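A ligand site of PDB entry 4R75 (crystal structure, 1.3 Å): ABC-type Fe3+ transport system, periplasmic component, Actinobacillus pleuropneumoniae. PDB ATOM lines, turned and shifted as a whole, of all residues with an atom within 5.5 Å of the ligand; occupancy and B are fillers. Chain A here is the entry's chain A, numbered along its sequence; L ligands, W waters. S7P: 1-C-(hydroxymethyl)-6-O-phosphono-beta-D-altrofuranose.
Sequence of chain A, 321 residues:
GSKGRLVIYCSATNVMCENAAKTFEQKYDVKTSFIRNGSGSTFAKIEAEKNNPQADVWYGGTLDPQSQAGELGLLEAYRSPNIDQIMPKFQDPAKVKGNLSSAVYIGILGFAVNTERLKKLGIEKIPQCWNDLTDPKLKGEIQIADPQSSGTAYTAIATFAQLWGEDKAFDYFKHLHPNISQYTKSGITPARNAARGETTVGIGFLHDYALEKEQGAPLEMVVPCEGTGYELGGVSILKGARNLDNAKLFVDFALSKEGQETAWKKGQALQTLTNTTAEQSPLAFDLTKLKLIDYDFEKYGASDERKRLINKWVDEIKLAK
The backbone NH of Ile 188 lies close to the side-chain hydroxyl of Ser 186. The backbone carbonyl oxygen of Tyr 105 is in hydrogen-bond range of the backbone NH of Gly 233, 2.8 Å away. OH of Tyr 105 is in hydrogen-bond range of N of Gly 61 (3.0 Å). The backbone NH (N) of Ala 153 is in hydrogen-bond range of the side-chain hydroxyl (OG) of Ser 150 (3.1 Å). The side-chain hydroxyl of Thr 62 lies within hydrogen-bond range of the side-chain hydroxyl of Ser 39 (2.7 Å). N of Gly 38 sits at hydrogen-bond distance from OG of Ser 41. The side-chain hydroxyl (OG) of Ser 150 is in hydrogen-bond range of the backbone NH (N) of Thr 152, at 3.1 Å.
O of Ser 11 touches C5 of the ligand, 3.5 Å away. Thr 13 touches the ligand (CG2 to C1, 3.6 Å). Gly 38 touches the ligand. CA of Ser 186 touches O14 of the ligand, at 3.8 Å. CG2 of Ile 188 touches C1 of the ligand (3.8 Å). Phe 205 touches the ligand. Hydrophobic or aromatic side chains that line the ligand: Tyr 105, Ile 188, Phe 205 and His 207. 19 residues have an atom within 4 Å of the ligand: Ser 11, Thr 13, Gly 38, Ser 39, Gly 40, Gly 61, Thr 62, Tyr 105, Ser 150, Gly 151, Thr 152, Ser 186, Gly 187, Ile 188, Phe 205, His 207, Asp 208, Glu 231 and Gln 271. Along chain A the residues within 4 Å of the ligand span positions 11 to 271.
OH of Tyr 105 is in hydrogen-bond range of O4 of the ligand. A ring nitrogen (NE2) of His 207 sits at hydrogen-bond distance from an oxygen (O3) of the ligand, at 2.8 Å. N of Gly 187 lies within hydrogen-bond range of O14 of the ligand (2.8 Å). The side-chain amide nitrogen (NE2) of Gln 271 sits at hydrogen-bond distance from an oxygen (O3) of the ligand (3.2 Å). The side-chain hydroxyl (OG) of Ser 39 sits at hydrogen-bond distance from an oxygen (O6) of the ligand. N of Thr 152 sits at hydrogen-bond distance from O15 of the ligand, 2.9 Å away. N of Ser 39 sits at hydrogen-bond distance from O7 of the ligand (2.9 Å). OD1 of Asp 208 sits at hydrogen-bond distance from O1 of the ligand (2.6 Å). The backbone NH of Gly 40 lies within hydrogen-bond range of an oxygen (O13) of the ligand, at 3.1 Å. O13 of the ligand sits at hydrogen-bond distance from N of Gly 151 (2.8 Å). The side-chain hydroxyl of Ser 150 is in hydrogen-bond range of an oxygen (O15) of the ligand, 2.7 Å away. The backbone NH (N) of Thr 62 sits at hydrogen-bond distance from an oxygen (O6) of the ligand (3.0 Å). An oxygen (O4) of the ligand lies within hydrogen-bond range of the side-chain carboxylate (OE1) of Glu 231. The backbone NH (N) of Gly 61 sits close to an oxygen (O4) of the ligand, at 3.4 Å. An oxygen (O15) of the ligand lies within hydrogen-bond range of the side-chain hydroxyl of Thr 152 (2.7 Å).
Water W3 lies within hydrogen-bond range of an oxygen (O13) of the ligand (2.7 Å), the backbone NH (N) of Ser 41 (2.8 Å), the backbone NH (N) of Gly 40 (3.3 Å) and the backbone carbonyl oxygen (O) of Ser 149 (3.4 Å). Water W2 lies within hydrogen-bond range of an oxygen (O1) of the ligand, the side-chain hydroxyl (OG1) of Thr 13 and the side-chain amide nitrogen (NE2) of Gln 271. Water W1 lies within hydrogen-bond range of the side-chain hydroxyl (OG1) of Thr 152, an oxygen (O2) of the ligand and the backbone carbonyl oxygen (O) of Gly 187.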
ATOM      1  N   SER A  11       1.774   2.292  15.615  1.00  0.00           N
ATOM      2  CA  SER A  11       2.948   2.796  14.890  1.00  0.00           C
ATOM      3  C   SER A  11       4.178   2.893  15.775  1.00  0.00           C
ATOM      4  O   SER A  11       5.217   3.380  15.323  1.00  0.00           O
ATOM      5  CB  SER A  11       2.655   4.146  14.241  1.00  0.00           C
ATOM      6  OG  SER A  11       1.654   4.035  13.238  1.00  0.00           O
ATOM      7  N   ALA A  12       4.053   2.457  17.026  1.00  0.00           N
ATOM      8  CA  ALA A  12       5.235   2.312  17.888  1.00  0.00           C
ATOM      9  C   ALA A  12       5.938   0.999  17.532  1.00  0.00           C
ATOM     10  O   ALA A  12       5.528   0.305  16.593  1.00  0.00           O
ATOM     11  CB  ALA A  12       4.837   2.330  19.356  1.00  0.00           C
ATOM     12  N   THR A  13       6.994   0.653  18.262  1.00  0.00           N
ATOM     13  CA  THR A  13       7.682  -0.605  17.994  1.00  0.00           C
ATOM     14  C   THR A  13       6.776  -1.768  18.376  1.00  0.00           C
ATOM     15  O   THR A  13       5.894  -1.639  19.229  1.00  0.00           O
ATOM     16  CB  THR A  13       8.980  -0.740  18.800  1.00  0.00           C
ATOM     17  OG1 THR A  13       8.711  -0.465  20.172  1.00  0.00           O
ATOM     18  CG2 THR A  13      10.070   0.207  18.269  1.00  0.00           C
ATOM     19  N   ARG A  36       1.005  -3.424  13.126  1.00  0.00           N
ATOM     20  CA  ARG A  36       2.002  -2.363  13.169  1.00  0.00           C
ATOM     21  C   ARG A  36       2.478  -1.932  11.789  1.00  0.00           C
ATOM     22  O   ARG A  36       2.862  -2.763  10.963  1.00  0.00           O
ATOM     23  CB  ARG A  36       3.213  -2.786  14.012  1.00  0.00           C
ATOM     24  CG  ARG A  36       4.271  -1.681  14.014  1.00  0.00           C
ATOM     25  CD  ARG A  36       5.638  -2.107  14.500  1.00  0.00           C
ATOM     26  NE  ARG A  36       6.545  -0.970  14.364  1.00  0.00           N
ATOM     27  CZ  ARG A  36       7.205  -0.667  13.252  1.00  0.00           C
ATOM     28  NH1 ARG A  36       7.077  -1.438  12.185  1.00  0.00           N
ATOM     29  NH2 ARG A  36       7.992   0.405  13.198  1.00  0.00           N
ATOM     30  N   GLY A  38       4.664   1.923  10.303  1.00  0.00           N
ATOM     31  CA  GLY A  38       5.156   3.236  10.692  1.00  0.00           C
ATOM     32  C   GLY A  38       4.085   4.295  10.565  1.00  0.00           C
ATOM     33  O   GLY A  38       3.033   4.066   9.982  1.00  0.00           O
ATOM     34  N   SER A  39       4.354   5.487  11.067  1.00  0.00           N
ATOM     35  CA  SER A  39       3.331   6.534  11.039  1.00  0.00           C
ATOM     36  C   SER A  39       3.051   7.025   9.622  1.00  0.00           C
ATOM     37  O   SER A  39       1.925   7.386   9.286  1.00  0.00           O
ATOM     38  CB  SER A  39       3.699   7.677  11.985  1.00  0.00           C
ATOM     39  OG  SER A  39       4.938   8.254  11.627  1.00  0.00           O
ATOM     40  N   GLY A  40       4.070   7.043   8.769  1.00  0.00           N
ATOM     41  CA  GLY A  40       3.866   7.450   7.392  1.00  0.00           C
ATOM     42  C   GLY A  40       2.979   6.459   6.653  1.00  0.00           C
ATOM     43  O   GLY A  40       1.997   6.849   6.003  1.00  0.00           O
ATOM     44  N   SER A  41       3.297   5.172   6.766  1.00  0.00           N
ATOM     45  CA  SER A  41       2.559   4.124   6.066  1.00  0.00           C
ATOM     46  C   SER A  41       1.201   3.785   6.696  1.00  0.00           C
ATOM     47  O   SER A  41       0.363   3.138   6.078  1.00  0.00           O
ATOM     48  CB  SER A  41       3.400   2.851   5.926  1.00  0.00           C
ATOM     49  OG  SER A  41       3.597   2.218   7.177  1.00  0.00           O
ATOM     50  N   GLY A  60       0.380   5.453  18.830  1.00  0.00           N
ATOM     51  CA  GLY A  60       1.807   5.661  18.630  1.00  0.00           C
ATOM     52  C   GLY A  60       2.119   6.177  17.246  1.00  0.00           C
ATOM     53  O   GLY A  60       1.216   6.350  16.407  1.00  0.00           O
ATOM     54  N   GLY A  61       3.406   6.428  17.002  1.00  0.00           N
ATOM     55  CA  GLY A  61       3.850   7.027  15.738  1.00  0.00           C
ATOM     56  C   GLY A  61       3.869   8.536  15.827  1.00  0.00           C
ATOM     57  O   GLY A  61       3.164   9.141  16.629  1.00  0.00           O
ATOM     58  N   THR A  62       4.681   9.166  14.974  1.00  0.00           N
ATOM     59  CA  THR A  62       4.806  10.614  14.975  1.00  0.00           C
ATOM     60  C   THR A  62       3.454  11.281  14.784  1.00  0.00           C
ATOM     61  O   THR A  62       2.553  10.759  14.117  1.00  0.00           O
ATOM     62  CB  THR A  62       5.763  11.124  13.888  1.00  0.00           C
ATOM     63  OG1 THR A  62       5.237  10.795  12.605  1.00  0.00           O
ATOM     64  CG2 THR A  62       7.160  10.543  14.031  1.00  0.00           C
ATOM     65  N   TYR A 105       3.620  10.422  24.023  1.00  0.00           N
ATOM     66  CA  TYR A 105       5.043  10.442  24.381  1.00  0.00           C
ATOM     67  C   TYR A 105       5.814  11.499  23.578  1.00  0.00           C
ATOM     68  O   TYR A 105       5.250  12.095  22.644  1.00  0.00           O
ATOM     69  CB  TYR A 105       5.696   9.056  24.212  1.00  0.00           C
ATOM     70  CG  TYR A 105       5.631   8.416  22.827  1.00  0.00           C
ATOM     71  CD1 TYR A 105       6.366   8.910  21.748  1.00  0.00           C
ATOM     72  CD2 TYR A 105       4.872   7.274  22.621  1.00  0.00           C
ATOM     73  CE1 TYR A 105       6.317   8.289  20.497  1.00  0.00           C
ATOM     74  CE2 TYR A 105       4.815   6.645  21.397  1.00  0.00           C
ATOM     75  CZ  TYR A 105       5.534   7.162  20.343  1.00  0.00           C
ATOM     76  OH  TYR A 105       5.467   6.529  19.134  1.00  0.00           O
ATOM     77  N   ALA A 145      15.746   7.643   7.441  1.00  0.00           N
ATOM     78  CA  ALA A 145      14.594   7.207   6.693  1.00  0.00           C
ATOM     79  C   ALA A 145      14.241   8.171   5.555  1.00  0.00           C
ATOM     80  O   ALA A 145      14.712   9.308   5.506  1.00  0.00           O
ATOM     81  CB  ALA A 145      13.399   6.987   7.611  1.00  0.00           C
ATOM     82  N   SER A 149       8.315   8.392   2.622  1.00  0.00           N
ATOM     83  CA  SER A 149       7.564   7.313   3.243  1.00  0.00           C
ATOM     84  C   SER A 149       7.442   7.418   4.763  1.00  0.00           C
ATOM     85  O   SER A 149       6.458   6.941   5.336  1.00  0.00           O
ATOM     86  CB  SER A 149       8.189   5.960   2.862  1.00  0.00           C
ATOM     87  OG  SER A 149       9.484   5.829   3.422  1.00  0.00           O
ATOM     88  N   SER A 150       8.412   8.037   5.408  1.00  0.00           N
ATOM     89  CA  SER A 150       8.561   7.910   6.852  1.00  0.00           C
ATOM     90  C   SER A 150       8.169   9.170   7.644  1.00  0.00           C
ATOM     91  O   SER A 150       8.609  10.278   7.323  1.00  0.00           O
ATOM     92  CB  SER A 150      10.015   7.532   7.147  1.00  0.00           C
ATOM     93  OG  SER A 150      10.394   7.850   8.480  1.00  0.00           O
ATOM     94  N   GLY A 151       7.414   8.962   8.714  1.00  0.00           N
ATOM     95  CA  GLY A 151       7.105  10.035   9.638  1.00  0.00           C
ATOM     96  C   GLY A 151       8.333  10.567  10.341  1.00  0.00           C
ATOM     97  O   GLY A 151       8.454  11.774  10.557  1.00  0.00           O
ATOM     98  N   THR A 152       9.245   9.680  10.712  1.00  0.00           N
ATOM     99  CA  THR A 152      10.504  10.074  11.364  1.00  0.00           C
ATOM    100  C   THR A 152      11.275  11.028  10.464  1.00  0.00           C
ATOM    101  O   THR A 152      11.804  12.058  10.915  1.00  0.00           O
ATOM    102  CB  THR A 152      11.348   8.826  11.648  1.00  0.00           C
ATOM    103  OG1 THR A 152      10.576   7.940  12.460  1.00  0.00           O
ATOM    104  CG2 THR A 152      12.639   9.180  12.359  1.00  0.00           C
ATOM    105  N   ALA A 153      11.365  10.695   9.180  1.00  0.00           N
ATOM    106  CA  ALA A 153      12.092  11.542   8.259  1.00  0.00           C
ATOM    107  C   ALA A 153      11.420  12.895   8.078  1.00  0.00           C
ATOM    108  O   ALA A 153      12.103  13.930   7.934  1.00  0.00           O
ATOM    109  CB  ALA A 153      12.257  10.841   6.913  1.00  0.00           C
ATOM    110  N   LYS A 185      12.902   2.804   4.370  1.00  0.00           N
ATOM    111  CA  LYS A 185      11.455   2.965   4.388  1.00  0.00           C
ATOM    112  C   LYS A 185      10.936   3.123   5.808  1.00  0.00           C
ATOM    113  O   LYS A 185      10.010   3.881   6.046  1.00  0.00           O
ATOM    114  CB  LYS A 185      10.755   1.787   3.698  1.00  0.00           C
ATOM    115  CG  LYS A 185      11.106   1.621   2.218  1.00  0.00           C
ATOM    116  CD  LYS A 185      10.613   2.784   1.386  1.00  0.00           C
ATOM    117  CE  LYS A 185      10.692   2.450  -0.108  1.00  0.00           C
ATOM    118  NZ  LYS A 185      12.078   2.121  -0.551  1.00  0.00           N
ATOM    119  N   SER A 186      11.550   2.417   6.752  1.00  0.00           N
ATOM    120  CA  SER A 186      11.164   2.516   8.157  1.00  0.00           C
ATOM    121  C   SER A 186      12.033   3.522   8.903  1.00  0.00           C
ATOM    122  O   SER A 186      13.264   3.566   8.731  1.00  0.00           O
ATOM    123  CB  SER A 186      11.252   1.165   8.871  1.00  0.00           C
ATOM    124  OG  SER A 186      11.020   1.287  10.276  1.00  0.00           O
ATOM    125  N   GLY A 187      11.394   4.322   9.748  1.00  0.00           N
ATOM    126  CA  GLY A 187      12.105   5.272  10.588  1.00  0.00           C
ATOM    127  C   GLY A 187      13.116   4.619  11.504  1.00  0.00           C
ATOM    128  O   GLY A 187      14.106   5.244  11.842  1.00  0.00           O
ATOM    129  N   ILE A 188      12.869   3.367  11.897  1.00  0.00           N
ATOM    130  CA  ILE A 188      13.734   2.706  12.871  1.00  0.00           C
ATOM    131  C   ILE A 188      14.901   1.885  12.280  1.00  0.00           C
ATOM    132  O   ILE A 188      15.783   1.419  13.015  1.00  0.00           O
ATOM    133  CB  ILE A 188      12.930   1.830  13.862  1.00  0.00           C
ATOM    134  CG1 ILE A 188      12.334   0.604  13.157  1.00  0.00           C
ATOM    135  CG2 ILE A 188      11.879   2.658  14.600  1.00  0.00           C
ATOM    136  CD1 ILE A 188      11.578  -0.335  14.092  1.00  0.00           C
ATOM    137  N   PHE A 205      15.058   8.800  16.170  1.00  0.00           N
ATOM    138  CA  PHE A 205      14.677   9.182  17.519  1.00  0.00           C
ATOM    139  C   PHE A 205      15.525   8.437  18.525  1.00  0.00           C
ATOM    140  O   PHE A 205      15.691   7.210  18.465  1.00  0.00           O
ATOM    141  CB  PHE A 205      13.192   8.895  17.732  1.00  0.00           C
ATOM    142  CG  PHE A 205      12.306   9.737  16.854  1.00  0.00           C
ATOM    143  CD1 PHE A 205      12.497  11.108  16.793  1.00  0.00           C
ATOM    144  CD2 PHE A 205      11.326   9.158  16.058  1.00  0.00           C
ATOM    145  CE1 PHE A 205      11.691  11.900  15.960  1.00  0.00           C
ATOM    146  CE2 PHE A 205      10.511   9.941  15.252  1.00  0.00           C
ATOM    147  CZ  PHE A 205      10.694  11.317  15.201  1.00  0.00           C
ATOM    148  N   HIS A 207      15.534   7.448  21.623  1.00  0.00           N
ATOM    149  CA  HIS A 207      15.125   6.328  22.480  1.00  0.00           C
ATOM    150  C   HIS A 207      15.327   4.975  21.793  1.00  0.00           C
ATOM    151  O   HIS A 207      15.590   3.970  22.485  1.00  0.00           O
ATOM    152  CB  HIS A 207      13.675   6.492  22.965  1.00  0.00           C
ATOM    153  CG  HIS A 207      12.701   6.637  21.850  1.00  0.00           C
ATOM    154  ND1 HIS A 207      12.321   7.872  21.368  1.00  0.00           N
ATOM    155  CD2 HIS A 207      12.006   5.714  21.139  1.00  0.00           C
ATOM    156  CE1 HIS A 207      11.457   7.697  20.387  1.00  0.00           C
ATOM    157  NE2 HIS A 207      11.241   6.400  20.227  1.00  0.00           N
ATOM    158  N   ASP A 208      15.220   4.925  20.472  1.00  0.00           N
ATOM    159  CA  ASP A 208      15.429   3.661  19.765  1.00  0.00           C
ATOM    160  C   ASP A 208      16.876   3.238  19.826  1.00  0.00           C
ATOM    161  O   ASP A 208      17.185   2.042  19.964  1.00  0.00           O
ATOM    162  CB  ASP A 208      14.963   3.759  18.316  1.00  0.00           C
ATOM    163  CG  ASP A 208      13.467   3.960  18.200  1.00  0.00           C
ATOM    164  OD1 ASP A 208      12.703   3.254  18.903  1.00  0.00           O
ATOM    165  OD2 ASP A 208      13.018   4.834  17.420  1.00  0.00           O
ATOM    166  N   GLU A 231       9.559  14.428  18.021  1.00  0.00           N
ATOM    167  CA  GLU A 231       8.183  14.024  17.726  1.00  0.00           C
ATOM    168  C   GLU A 231       7.361  14.041  19.001  1.00  0.00           C
ATOM    169  O   GLU A 231       7.893  13.914  20.120  1.00  0.00           O
ATOM    170  CB  GLU A 231       8.137  12.583  17.196  1.00  0.00           C
ATOM    171  CG  GLU A 231       8.782  11.568  18.169  1.00  0.00           C
ATOM    172  CD  GLU A 231       8.336  10.135  17.975  1.00  0.00           C
ATOM    173  OE1 GLU A 231       7.340   9.902  17.252  1.00  0.00           O
ATOM    174  OE2 GLU A 231       9.015   9.247  18.548  1.00  0.00           O
ATOM    175  N   GLY A 233       4.390  11.371  20.058  1.00  0.00           N
ATOM    176  CA  GLY A 233       3.649  10.179  19.682  1.00  0.00           C
ATOM    177  C   GLY A 233       2.170  10.490  19.824  1.00  0.00           C
ATOM    178  O   GLY A 233       1.759  11.147  20.769  1.00  0.00           O
ATOM    179  N   GLN A 271      10.679   6.237  25.230  1.00  0.00           N
ATOM    180  CA  GLN A 271      10.259   7.613  25.012  1.00  0.00           C
ATOM    181  C   GLN A 271       9.987   8.294  26.327  1.00  0.00           C
ATOM    182  O   GLN A 271       9.758   7.657  27.354  1.00  0.00           O
ATOM    183  CB  GLN A 271       9.007   7.694  24.124  1.00  0.00           C
ATOM    184  CG  GLN A 271       9.156   7.049  22.755  1.00  0.00           C
ATOM    185  CD  GLN A 271       8.568   5.638  22.727  1.00  0.00           C
ATOM    186  OE1 GLN A 271       8.429   4.990  23.767  1.00  0.00           O
ATOM    187  NE2 GLN A 271       8.206   5.163  21.532  1.00  0.00           N
HETATM  188  O1  S7P L   1      10.158   3.806  18.834  1.00  0.00           O
HETATM  189  C1  S7P L   1       9.670   3.716  17.477  1.00  0.00           C
HETATM  190  C2  S7P L   1       9.439   5.122  16.882  1.00  0.00           C
HETATM  191  O2  S7P L   1      10.607   5.829  16.787  1.00  0.00           O
HETATM  192  O5  S7P L   1       8.835   4.950  15.570  1.00  0.00           O
HETATM  193  C5  S7P L   1       7.682   5.819  15.433  1.00  0.00           C
HETATM  194  C6  S7P L   1       7.695   6.359  14.061  1.00  0.00           C
HETATM  195  O6  S7P L   1       6.539   7.113  13.822  1.00  0.00           O
HETATM  196  C7  S7P L   1       7.771   5.206  12.919  1.00  0.00           C
HETATM  197  O7  S7P L   1       7.161   5.689  11.745  1.00  0.00           O
HETATM  198  P12 S7P L   1       7.988   5.790  10.392  1.00  0.00           P
HETATM  199  O13 S7P L   1       6.976   6.242   9.381  1.00  0.00           O
HETATM  200  O14 S7P L   1       8.568   4.426  10.077  1.00  0.00           O
HETATM  201  O15 S7P L   1       9.095   6.823  10.553  1.00  0.00           O
HETATM  202  C4  S7P L   1       7.890   6.820  16.548  1.00  0.00           C
HETATM  203  O4  S7P L   1       6.603   7.472  16.935  1.00  0.00           O
HETATM  204  C3  S7P L   1       8.396   5.936  17.614  1.00  0.00           C
HETATM  205  O3  S7P L   1       8.904   6.607  18.750  1.00  0.00           O
HETATM  206  O   HOH W   1      11.708   6.004  14.051  1.00  0.00           O
HETATM  207  O   HOH W   2       8.246   2.417  20.423  1.00  0.00           O
HETATM  208  O   HOH W   3       5.890   4.500   7.655  1.00  0.00           O
HETATM  209  O   HOH W   4       7.729   2.380  15.240  1.00  0.00           O
